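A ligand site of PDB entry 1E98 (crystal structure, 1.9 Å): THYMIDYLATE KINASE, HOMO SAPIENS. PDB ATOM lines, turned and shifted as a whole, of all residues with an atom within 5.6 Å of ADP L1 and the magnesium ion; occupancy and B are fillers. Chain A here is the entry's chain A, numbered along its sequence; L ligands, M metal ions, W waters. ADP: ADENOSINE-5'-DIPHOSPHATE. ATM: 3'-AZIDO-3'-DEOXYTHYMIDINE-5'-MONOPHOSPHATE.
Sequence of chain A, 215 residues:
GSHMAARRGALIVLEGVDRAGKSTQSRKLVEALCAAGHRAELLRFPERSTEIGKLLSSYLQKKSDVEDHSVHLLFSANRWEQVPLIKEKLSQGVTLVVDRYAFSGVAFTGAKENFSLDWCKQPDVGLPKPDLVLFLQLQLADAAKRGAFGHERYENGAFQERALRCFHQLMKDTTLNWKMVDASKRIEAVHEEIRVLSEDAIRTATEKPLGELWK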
ATOM      1  N   VAL A  17       8.470  16.943  -4.338  1.00  0.00           N
ATOM      2  CA  VAL A  17       7.263  16.207  -4.752  1.00  0.00           C
ATOM      3  C   VAL A  17       7.422  14.735  -4.450  1.00  0.00           C
ATOM      4  O   VAL A  17       8.426  14.241  -3.928  1.00  0.00           O
ATOM      5  CB  VAL A  17       6.866  16.507  -6.208  1.00  0.00           C
ATOM      6  CG1 VAL A  17       6.907  18.027  -6.417  1.00  0.00           C
ATOM      7  CG2 VAL A  17       7.774  15.779  -7.172  1.00  0.00           C
ATOM      8  N   ASP A  18       6.348  14.002  -4.728  1.00  0.00           N
ATOM      9  CA  ASP A  18       6.256  12.586  -4.364  1.00  0.00           C
ATOM     10  C   ASP A  18       7.276  11.777  -5.132  1.00  0.00           C
ATOM     11  O   ASP A  18       7.394  11.940  -6.347  1.00  0.00           O
ATOM     12  CB  ASP A  18       4.798  12.144  -4.611  1.00  0.00           C
ATOM     13  CG  ASP A  18       4.553  10.713  -4.176  1.00  0.00           C
ATOM     14  OD1 ASP A  18       4.881  10.346  -3.028  1.00  0.00           O
ATOM     15  OD2 ASP A  18       4.058   9.927  -5.002  1.00  0.00           O
ATOM     16  N   ARG A  19       8.046  10.979  -4.400  1.00  0.00           N
ATOM     17  CA  ARG A  19       9.020  10.081  -5.004  1.00  0.00           C
ATOM     18  C   ARG A  19      10.231  10.811  -5.529  1.00  0.00           C
ATOM     19  O   ARG A  19      11.084  10.235  -6.212  1.00  0.00           O
ATOM     20  CB  ARG A  19       8.330   9.286  -6.136  1.00  0.00           C
ATOM     21  CG  ARG A  19       7.363   8.207  -5.646  1.00  0.00           C
ATOM     22  CD  ARG A  19       6.580   7.563  -6.774  1.00  0.00           C
ATOM     23  NE  ARG A  19       5.555   8.382  -7.375  1.00  0.00           N
ATOM     24  CZ  ARG A  19       4.926   8.138  -8.516  1.00  0.00           C
ATOM     25  NH1 ARG A  19       5.226   7.037  -9.208  1.00  0.00           N
ATOM     26  NH2 ARG A  19       3.994   8.979  -8.970  1.00  0.00           N
ATOM     27  N   ALA A  20      10.324  12.089  -5.130  1.00  0.00           N
ATOM     28  CA  ALA A  20      11.429  12.905  -5.622  1.00  0.00           C
ATOM     29  C   ALA A  20      12.751  12.542  -4.977  1.00  0.00           C
ATOM     30  O   ALA A  20      13.767  12.710  -5.668  1.00  0.00           O
ATOM     31  CB  ALA A  20      11.086  14.382  -5.484  1.00  0.00           C
ATOM     32  N   GLY A  21      12.704  11.863  -3.827  1.00  0.00           N
ATOM     33  CA  GLY A  21      13.969  11.439  -3.201  1.00  0.00           C
ATOM     34  C   GLY A  21      14.298  12.154  -1.897  1.00  0.00           C
ATOM     35  O   GLY A  21      15.446  12.252  -1.484  1.00  0.00           O
ATOM     36  N   LYS A  22      13.362  12.699  -1.152  1.00  0.00           N
ATOM     37  CA  LYS A  22      13.655  13.372   0.121  1.00  0.00           C
ATOM     38  C   LYS A  22      14.391  12.467   1.088  1.00  0.00           C
ATOM     39  O   LYS A  22      15.359  12.840   1.737  1.00  0.00           O
ATOM     40  CB  LYS A  22      12.331  13.885   0.730  1.00  0.00           C
ATOM     41  CG  LYS A  22      11.606  14.894  -0.204  1.00  0.00           C
ATOM     42  CD  LYS A  22      10.255  15.339   0.349  1.00  0.00           C
ATOM     43  CE  LYS A  22       9.203  14.247   0.436  1.00  0.00           C
ATOM     44  NZ  LYS A  22       8.834  13.632  -0.877  1.00  0.00           N
ATOM     45  N   SER A  23      13.880  11.261   1.316  1.00  0.00           N
ATOM     46  CA  SER A  23      14.451  10.312   2.258  1.00  0.00           C
ATOM     47  C   SER A  23      15.790   9.780   1.774  1.00  0.00           C
ATOM     48  O   SER A  23      16.735   9.804   2.542  1.00  0.00           O
ATOM     49  CB  SER A  23      13.501   9.113   2.452  1.00  0.00           C
ATOM     50  OG  SER A  23      12.327   9.742   2.941  1.00  0.00           O
ATOM     51  N   THR A  24      15.840   9.400   0.490  1.00  0.00           N
ATOM     52  CA  THR A  24      17.157   8.936   0.028  1.00  0.00           C
ATOM     53  C   THR A  24      18.221  10.021   0.160  1.00  0.00           C
ATOM     54  O   THR A  24      19.314   9.791   0.670  1.00  0.00           O
ATOM     55  CB  THR A  24      17.062   8.475  -1.434  1.00  0.00           C
ATOM     56  OG1 THR A  24      16.118   7.420  -1.592  1.00  0.00           O
ATOM     57  CG2 THR A  24      18.427   8.077  -1.965  1.00  0.00           C
ATOM     58  N   GLN A  25      17.902  11.222  -0.342  1.00  0.00           N
ATOM     59  CA  GLN A  25      18.855  12.323  -0.302  1.00  0.00           C
ATOM     60  C   GLN A  25      19.148  12.738   1.148  1.00  0.00           C
ATOM     61  O   GLN A  25      20.291  13.116   1.464  1.00  0.00           O
ATOM     62  CB  GLN A  25      18.409  13.534  -1.143  1.00  0.00           C
ATOM     63  CG  GLN A  25      18.314  13.239  -2.648  1.00  0.00           C
ATOM     64  CD  GLN A  25      19.584  12.623  -3.205  1.00  0.00           C
ATOM     65  OE1 GLN A  25      20.666  12.887  -2.690  1.00  0.00           O
ATOM     66  NE2 GLN A  25      19.546  11.765  -4.229  1.00  0.00           N
ATOM     67  N   ARG A  27      19.260  10.823   3.842  1.00  0.00           N
ATOM     68  CA  ARG A  27      20.191   9.856   4.476  1.00  0.00           C
ATOM     69  C   ARG A  27      21.558  10.022   3.855  1.00  0.00           C
ATOM     70  O   ARG A  27      22.576  10.021   4.553  1.00  0.00           O
ATOM     71  CB  ARG A  27      19.732   8.392   4.170  1.00  0.00           C
ATOM     72  CG  ARG A  27      18.388   7.974   4.786  1.00  0.00           C
ATOM     73  CD  ARG A  27      18.122   6.484   4.516  1.00  0.00           C
ATOM     74  NE  ARG A  27      18.029   6.131   3.077  1.00  0.00           N
ATOM     75  CZ  ARG A  27      16.823   6.143   2.479  1.00  0.00           C
ATOM     76  NH1 ARG A  27      15.701   6.439   3.142  1.00  0.00           N
ATOM     77  NH2 ARG A  27      16.713   5.886   1.192  1.00  0.00           N
ATOM     78  N   ASP A  99      13.878  15.570   6.924  1.00  0.00           N
ATOM     79  CA  ASP A  99      13.081  15.009   5.854  1.00  0.00           C
ATOM     80  C   ASP A  99      11.628  15.459   6.054  1.00  0.00           C
ATOM     81  O   ASP A  99      10.959  14.778   6.809  1.00  0.00           O
ATOM     82  CB  ASP A  99      13.189  13.480   5.970  1.00  0.00           C
ATOM     83  CG  ASP A  99      12.533  12.681   4.866  1.00  0.00           C
ATOM     84  OD1 ASP A  99      11.751  13.283   4.081  1.00  0.00           O
ATOM     85  OD2 ASP A  99      12.816  11.436   4.845  1.00  0.00           O
ATOM     86  N   ARG A 100      11.244  16.542   5.426  1.00  0.00           N
ATOM     87  CA  ARG A 100       9.954  17.177   5.565  1.00  0.00           C
ATOM     88  C   ARG A 100       9.899  18.045   6.855  1.00  0.00           C
ATOM     89  O   ARG A 100      10.375  17.655   7.915  1.00  0.00           O
ATOM     90  CB  ARG A 100       8.744  16.269   5.568  1.00  0.00           C
ATOM     91  CG  ARG A 100       8.465  15.539   4.227  1.00  0.00           C
ATOM     92  CD  ARG A 100       7.065  14.894   4.452  1.00  0.00           C
ATOM     93  NE  ARG A 100       6.770  13.968   3.388  1.00  0.00           N
ATOM     94  CZ  ARG A 100       6.249  14.245   2.195  1.00  0.00           C
ATOM     95  NH1 ARG A 100       5.932  15.474   1.845  1.00  0.00           N
ATOM     96  NH2 ARG A 100       6.067  13.251   1.320  1.00  0.00           N
ATOM     97  N   ARG A 146       9.785   5.738 -11.063  1.00  0.00           N
ATOM     98  CA  ARG A 146      10.290   5.422  -9.754  1.00  0.00           C
ATOM     99  C   ARG A 146       9.353   4.491  -9.021  1.00  0.00           C
ATOM    100  O   ARG A 146       9.677   3.991  -7.941  1.00  0.00           O
ATOM    101  CB  ARG A 146      10.570   6.707  -8.936  1.00  0.00           C
ATOM    102  CG  ARG A 146      11.910   7.315  -9.353  1.00  0.00           C
ATOM    103  CD  ARG A 146      12.085   8.723  -8.780  1.00  0.00           C
ATOM    104  NE  ARG A 146      12.999   9.481  -9.626  1.00  0.00           N
ATOM    105  CZ  ARG A 146      13.679  10.573  -9.275  1.00  0.00           C
ATOM    106  NH1 ARG A 146      13.529  11.003  -8.035  1.00  0.00           N
ATOM    107  NH2 ARG A 146      14.484  11.188 -10.130  1.00  0.00           N
ATOM    108  N   ALA A 183      15.634  17.128  -9.115  1.00  0.00           N
ATOM    109  CA  ALA A 183      15.721  15.755  -8.574  1.00  0.00           C
ATOM    110  C   ALA A 183      15.532  14.668  -9.608  1.00  0.00           C
ATOM    111  O   ALA A 183      15.509  13.476  -9.279  1.00  0.00           O
ATOM    112  CB  ALA A 183      14.760  15.614  -7.402  1.00  0.00           C
ATOM    113  N   SER A 184      15.532  15.045 -10.893  1.00  0.00           N
ATOM    114  CA  SER A 184      15.426  14.064 -11.974  1.00  0.00           C
ATOM    115  C   SER A 184      16.726  13.358 -12.316  1.00  0.00           C
ATOM    116  O   SER A 184      16.737  12.366 -13.079  1.00  0.00           O
ATOM    117  CB  SER A 184      14.854  14.738 -13.235  1.00  0.00           C
ATOM    118  OG  SER A 184      15.706  15.656 -13.879  1.00  0.00           O
ATOM    119  N   LYS A 185      17.850  13.911 -11.879  1.00  0.00           N
ATOM    120  CA  LYS A 185      19.152  13.347 -12.168  1.00  0.00           C
ATOM    121  C   LYS A 185      19.328  12.034 -11.396  1.00  0.00           C
ATOM    122  O   LYS A 185      18.380  11.646 -10.709  1.00  0.00           O
ATOM    123  CB  LYS A 185      20.267  14.325 -11.808  1.00  0.00           C
ATOM    124  CG  LYS A 185      20.232  15.690 -12.531  1.00  0.00           C
ATOM    125  CD  LYS A 185      20.889  16.733 -11.599  1.00  0.00           C
ATOM    126  CE  LYS A 185      21.490  17.877 -12.367  1.00  0.00           C
ATOM    127  NZ  LYS A 185      22.433  18.710 -11.586  1.00  0.00           N
ATOM    128  N   ARG A 186      20.502  11.407 -11.546  1.00  0.00           N
ATOM    129  CA  ARG A 186      20.704  10.159 -10.805  1.00  0.00           C
ATOM    130  C   ARG A 186      20.735  10.447  -9.295  1.00  0.00           C
ATOM    131  O   ARG A 186      20.981  11.587  -8.928  1.00  0.00           O
ATOM    132  CB  ARG A 186      22.061   9.509 -11.083  1.00  0.00           C
ATOM    133  CG  ARG A 186      23.288  10.352 -10.747  1.00  0.00           C
ATOM    134  CD  ARG A 186      23.943  10.743 -12.074  1.00  0.00           C
ATOM    135  NE  ARG A 186      25.405  10.795 -11.937  1.00  0.00           N
ATOM    136  CZ  ARG A 186      26.067   9.764 -11.408  1.00  0.00           C
ATOM    137  NH1 ARG A 186      25.402   8.686 -11.035  1.00  0.00           N
ATOM    138  NH2 ARG A 186      27.399   9.867 -11.286  1.00  0.00           N
ATOM    139  N   ILE A 187      20.707   9.386  -8.524  1.00  0.00           N
ATOM    140  CA  ILE A 187      20.804   9.546  -7.054  1.00  0.00           C
ATOM    141  C   ILE A 187      22.087  10.277  -6.697  1.00  0.00           C
ATOM    142  O   ILE A 187      22.069  11.262  -5.931  1.00  0.00           O
ATOM    143  CB  ILE A 187      20.672   8.177  -6.371  1.00  0.00           C
ATOM    144  CG1 ILE A 187      19.244   7.617  -6.393  1.00  0.00           C
ATOM    145  CG2 ILE A 187      21.222   8.243  -4.958  1.00  0.00           C
ATOM    146  CD1 ILE A 187      19.114   6.188  -5.884  1.00  0.00           C
ATOM    147  N   VAL A 190      22.132  14.118  -7.925  1.00  0.00           N
ATOM    148  CA  VAL A 190      21.266  14.941  -7.072  1.00  0.00           C
ATOM    149  C   VAL A 190      21.974  15.185  -5.739  1.00  0.00           C
ATOM    150  O   VAL A 190      22.003  16.290  -5.215  1.00  0.00           O
ATOM    151  CB  VAL A 190      19.912  14.235  -6.888  1.00  0.00           C
ATOM    152  CG1 VAL A 190      18.967  14.925  -5.924  1.00  0.00           C
ATOM    153  CG2 VAL A 190      19.284  14.202  -8.309  1.00  0.00           C
HETATM  154  PB  ADP L   1      10.600  10.411  -1.086  1.00  0.00           P
HETATM  155  O1B ADP L   1      10.763  11.752  -1.710  1.00  0.00           O
HETATM  156  O2B ADP L   1      11.049  10.288   0.334  1.00  0.00           O
HETATM  157  O3B ADP L   1       9.180   9.833  -1.256  1.00  0.00           O
HETATM  158  PA  ADP L   1      12.460   8.207  -1.713  1.00  0.00           P
HETATM  159  O1A ADP L   1      11.827   7.277  -0.781  1.00  0.00           O
HETATM  160  O2A ADP L   1      13.831   8.772  -1.419  1.00  0.00           O
HETATM  161  O3A ADP L   1      11.532   9.488  -2.066  1.00  0.00           O
HETATM  162  O5' ADP L   1      12.627   7.586  -3.156  1.00  0.00           O
HETATM  163  C5' ADP L   1      11.514   7.058  -3.922  1.00  0.00           C
HETATM  164  C4' ADP L   1      11.948   5.866  -4.759  1.00  0.00           C
HETATM  165  O4' ADP L   1      12.674   6.460  -5.841  1.00  0.00           O
HETATM  166  C3' ADP L   1      12.884   4.853  -4.086  1.00  0.00           C
HETATM  167  O3' ADP L   1      12.799   3.627  -4.803  1.00  0.00           O
HETATM  168  C2' ADP L   1      14.249   5.473  -4.414  1.00  0.00           C
HETATM  169  O2' ADP L   1      15.286   4.539  -4.525  1.00  0.00           O
HETATM  170  C1' ADP L   1      13.989   6.036  -5.827  1.00  0.00           C
HETATM  171  N9  ADP L   1      14.842   7.202  -6.142  1.00  0.00           N
HETATM  172  C8  ADP L   1      15.162   8.234  -5.277  1.00  0.00           C
HETATM  173  N7  ADP L   1      15.852   9.196  -5.873  1.00  0.00           N
HETATM  174  C5  ADP L   1      16.030   8.753  -7.190  1.00  0.00           C
HETATM  175  C6  ADP L   1      16.698   9.333  -8.266  1.00  0.00           C
HETATM  176  N6  ADP L   1      17.327  10.468  -8.271  1.00  0.00           N
HETATM  177  N1  ADP L   1      16.612   8.570  -9.371  1.00  0.00           N
HETATM  178  C2  ADP L   1      16.004   7.393  -9.474  1.00  0.00           C
HETATM  179  N3  ADP L   1      15.364   6.786  -8.471  1.00  0.00           N
HETATM  180  C4  ADP L   1      15.415   7.536  -7.396  1.00  0.00           C
HETATM  181  P   ATM L   2       6.537  10.547   4.008  1.00  0.00           P
HETATM  182  OP1 ATM L   2       6.236  10.612   2.546  1.00  0.00           O
HETATM  183  OP2 ATM L   2       7.709  11.483   4.373  1.00  0.00           O
HETATM  184  OP3 ATM L   2       6.754   9.109   4.492  1.00  0.00           O
HETATM  185  O5' ATM L   2       5.407  11.287   4.859  1.00  0.00           O
HETATM  186  C5' ATM L   2       4.077  10.882   4.976  1.00  0.00           C
HETATM  187  C4' ATM L   2       2.938  11.890   4.794  1.00  0.00           C
HETATM  188  O4' ATM L   2       2.575  12.908   5.707  1.00  0.00           O
HETATM  189  C3' ATM L   2       2.986  12.532   3.429  1.00  0.00           C
HETATM  190  N3' ATM L   2       1.658  12.102   2.833  1.00  0.00           N
HETATM  191  N4' ATM L   2       1.773  11.985   1.598  1.00  0.00           N
HETATM  192  N5' ATM L   2       2.241  11.977   0.564  1.00  0.00           N
HETATM  193  C2' ATM L   2       3.055  14.042   3.721  1.00  0.00           C
HETATM  194  C1' ATM L   2       2.358  14.147   5.082  1.00  0.00           C
HETATM  195  N1  ATM L   2       2.578  15.213   6.062  1.00  0.00           N
HETATM  196  C2  ATM L   2       1.443  16.003   6.414  1.00  0.00           C
HETATM  197  O2  ATM L   2       0.336  15.814   5.897  1.00  0.00           O
HETATM  198  N3  ATM L   2       1.656  17.008   7.333  1.00  0.00           N
HETATM  199  C4  ATM L   2       2.899  17.196   7.878  1.00  0.00           C
HETATM  200  O4  ATM L   2       3.054  18.190   8.835  1.00  0.00           O
HETATM  201  C5  ATM L   2       4.053  16.334   7.495  1.00  0.00           C
HETATM  202  C5A ATM L   2       5.403  16.557   8.103  1.00  0.00           C
HETATM  203  C6  ATM L   2       3.838  15.326   6.567  1.00  0.00           C
HETATM  204 MG    MG M   1      10.246   9.634   2.090  1.00  0.00          MG
HETATM  205  O   HOH W   1      16.792   9.196 -11.906  1.00  0.00           O
HETATM  206  O   HOH W   2       9.949  11.693   2.866  1.00  0.00           O
HETATM  207  O   HOH W   3       8.238   9.648   1.253  1.00  0.00           O
HETATM  208  O   HOH W   4      10.588   7.519   1.458  1.00  0.00           O
HETATM  209  O   HOH W   5      12.125   3.051  -7.784  1.00  0.00           O
HETATM  210  O   HOH W   6      16.636   3.529  -6.858  1.00  0.00           O
HETATM  211  O   HOH W   7       8.145   7.456  -1.829  1.00  0.00           O
HETATM  212  O   HOH W   8      16.708  11.637  -5.692  1.00  0.00           O
HETATM  213  O   HOH W   9      11.062   4.598  -0.877  1.00  0.00           O
HETATM  214  O   HOH W  10       7.096  11.511  -1.153  1.00  0.00           O
HETATM  215  O   HOH W  11      16.250   4.856  -2.312  1.00  0.00           O
HETATM  216  O   HOH W  12       9.502   8.914   3.947  1.00  0.00           O
HETATM  217  O   HOH W  13      10.796   2.763  -2.903  1.00  0.00           O
HETATM  218  O   HOH W  14      14.161   4.547  -9.402  1.00  0.00           O
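The side-chain hydroxyl of Thr 24 is in hydrogen-bond range of the guanidinium group of Arg 27, 3.2 Å away. The side-chain amino group of Lys 22 lies within hydrogen-bond range of the backbone carbonyl oxygen of Val 17 (3.1 Å). The guanidinium group (NH1) of Arg 146 sits at hydrogen-bond distance from the backbone carbonyl oxygen (O) of Ala 20, at 2.9 Å. The guanidinium group of Arg 19 lies within salt-bridge range of the side-chain carboxylate of Asp 18, at 3.2 Å. The backbone carbonyl oxygen (O) of Ile 187 is in hydrogen-bond range of the side-chain amide nitrogen (NE2) of Gln 25. O of Arg 19 lies close to NH1 of Arg 146 (3.1 Å). OG of Ser 23 lies close to OD2 of Asp 99 (2.6 Å). The backbone carbonyl oxygen (O) of Ala 183 sits at hydrogen-bond distance from the guanidinium group (NH2) of Arg 146 (2.6 Å).
One residue has an atom within 4 Å of the magnesium ion: Ser 23.
Residues that only touch ADP L1: Ile 187, Arg 19, Arg 186 and Ala 183. Hydrophobic or aromatic side chains that line ADP L1: Ile 187. 11 residues have an atom within 4 Å of ADP L1: Arg 19, Ala 20, Gly 21, Lys 22, Ser 23, Thr 24, Arg 146, Ala 183, Lys 185, Arg 186 and Ile 187.
Water W2 bridges the side-chain carboxylate (OD1) of Asp 99 (2.7 Å) and an oxygen (OP2) of ATM L2 (2.7 Å). Water W3 lies within hydrogen-bond range of OP1 of ATM L2 (2.6 Å) and O3B of ADP L1 (2.7 Å). Water W11 bridges O2' of ADP L1 (2.4 Å) and OG1 of Thr 24 (2.7 Å). Water W8 lies within hydrogen-bond range of N7 of ADP L1 (2.6 Å), O of Ala 20 (3.1 Å) and NE2 of Gln 25 (3.2 Å). Water W5 lies within hydrogen-bond range of the backbone carbonyl oxygen (O) of Arg 146 (2.6 Å) and an oxygen (O3') of ADP L1 (3.1 Å).
An oxygen (O2A) of ADP L1 is in hydrogen-bond range of the backbone NH (N) of Thr 24 (2.8 Å). The backbone NH of Gly 21 sits at hydrogen-bond distance from an oxygen (O1B) of ADP L1, at 2.9 Å. A nitrogen (N1) of ADP L1 sits close to the guanidinium group (NH2) of Arg 146, 3.5 Å away. An oxygen (O1B) of ADP L1 is in salt-bridge range of the side-chain amino group of Lys 22 (2.8 Å). O of Lys 185 is in hydrogen-bond range of N6 of ADP L1 (2.9 Å). The guanidinium group (NE) of Arg 100 lies within salt-bridge range of an oxygen (OP2) of ATM L2, 2.8 Å away. An oxygen (O2B) of ADP L1 sits close to the backbone NH (N) of Ser 23 (3.2 Å). N of Ala 20 sits at hydrogen-bond distance from O1B of ADP L1 (3.5 Å). An oxygen (O2A) of ADP L1 sits at hydrogen-bond distance from the side-chain hydroxyl (OG1) of Thr 24 (2.7 Å). N of Lys 22 lies within hydrogen-bond range of O1B of ADP L1 (2.8 Å).
The magnesium ion is bound by O2B of ADP L1 (2.0 Å), water W12 (2.1 Å), water W3 (2.2 Å), water W2 (2.2 Å), water W4 (2.2 Å) and OG of Ser 23 (2.3 Å). The magnesium ion has six donor atoms within binding distance.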
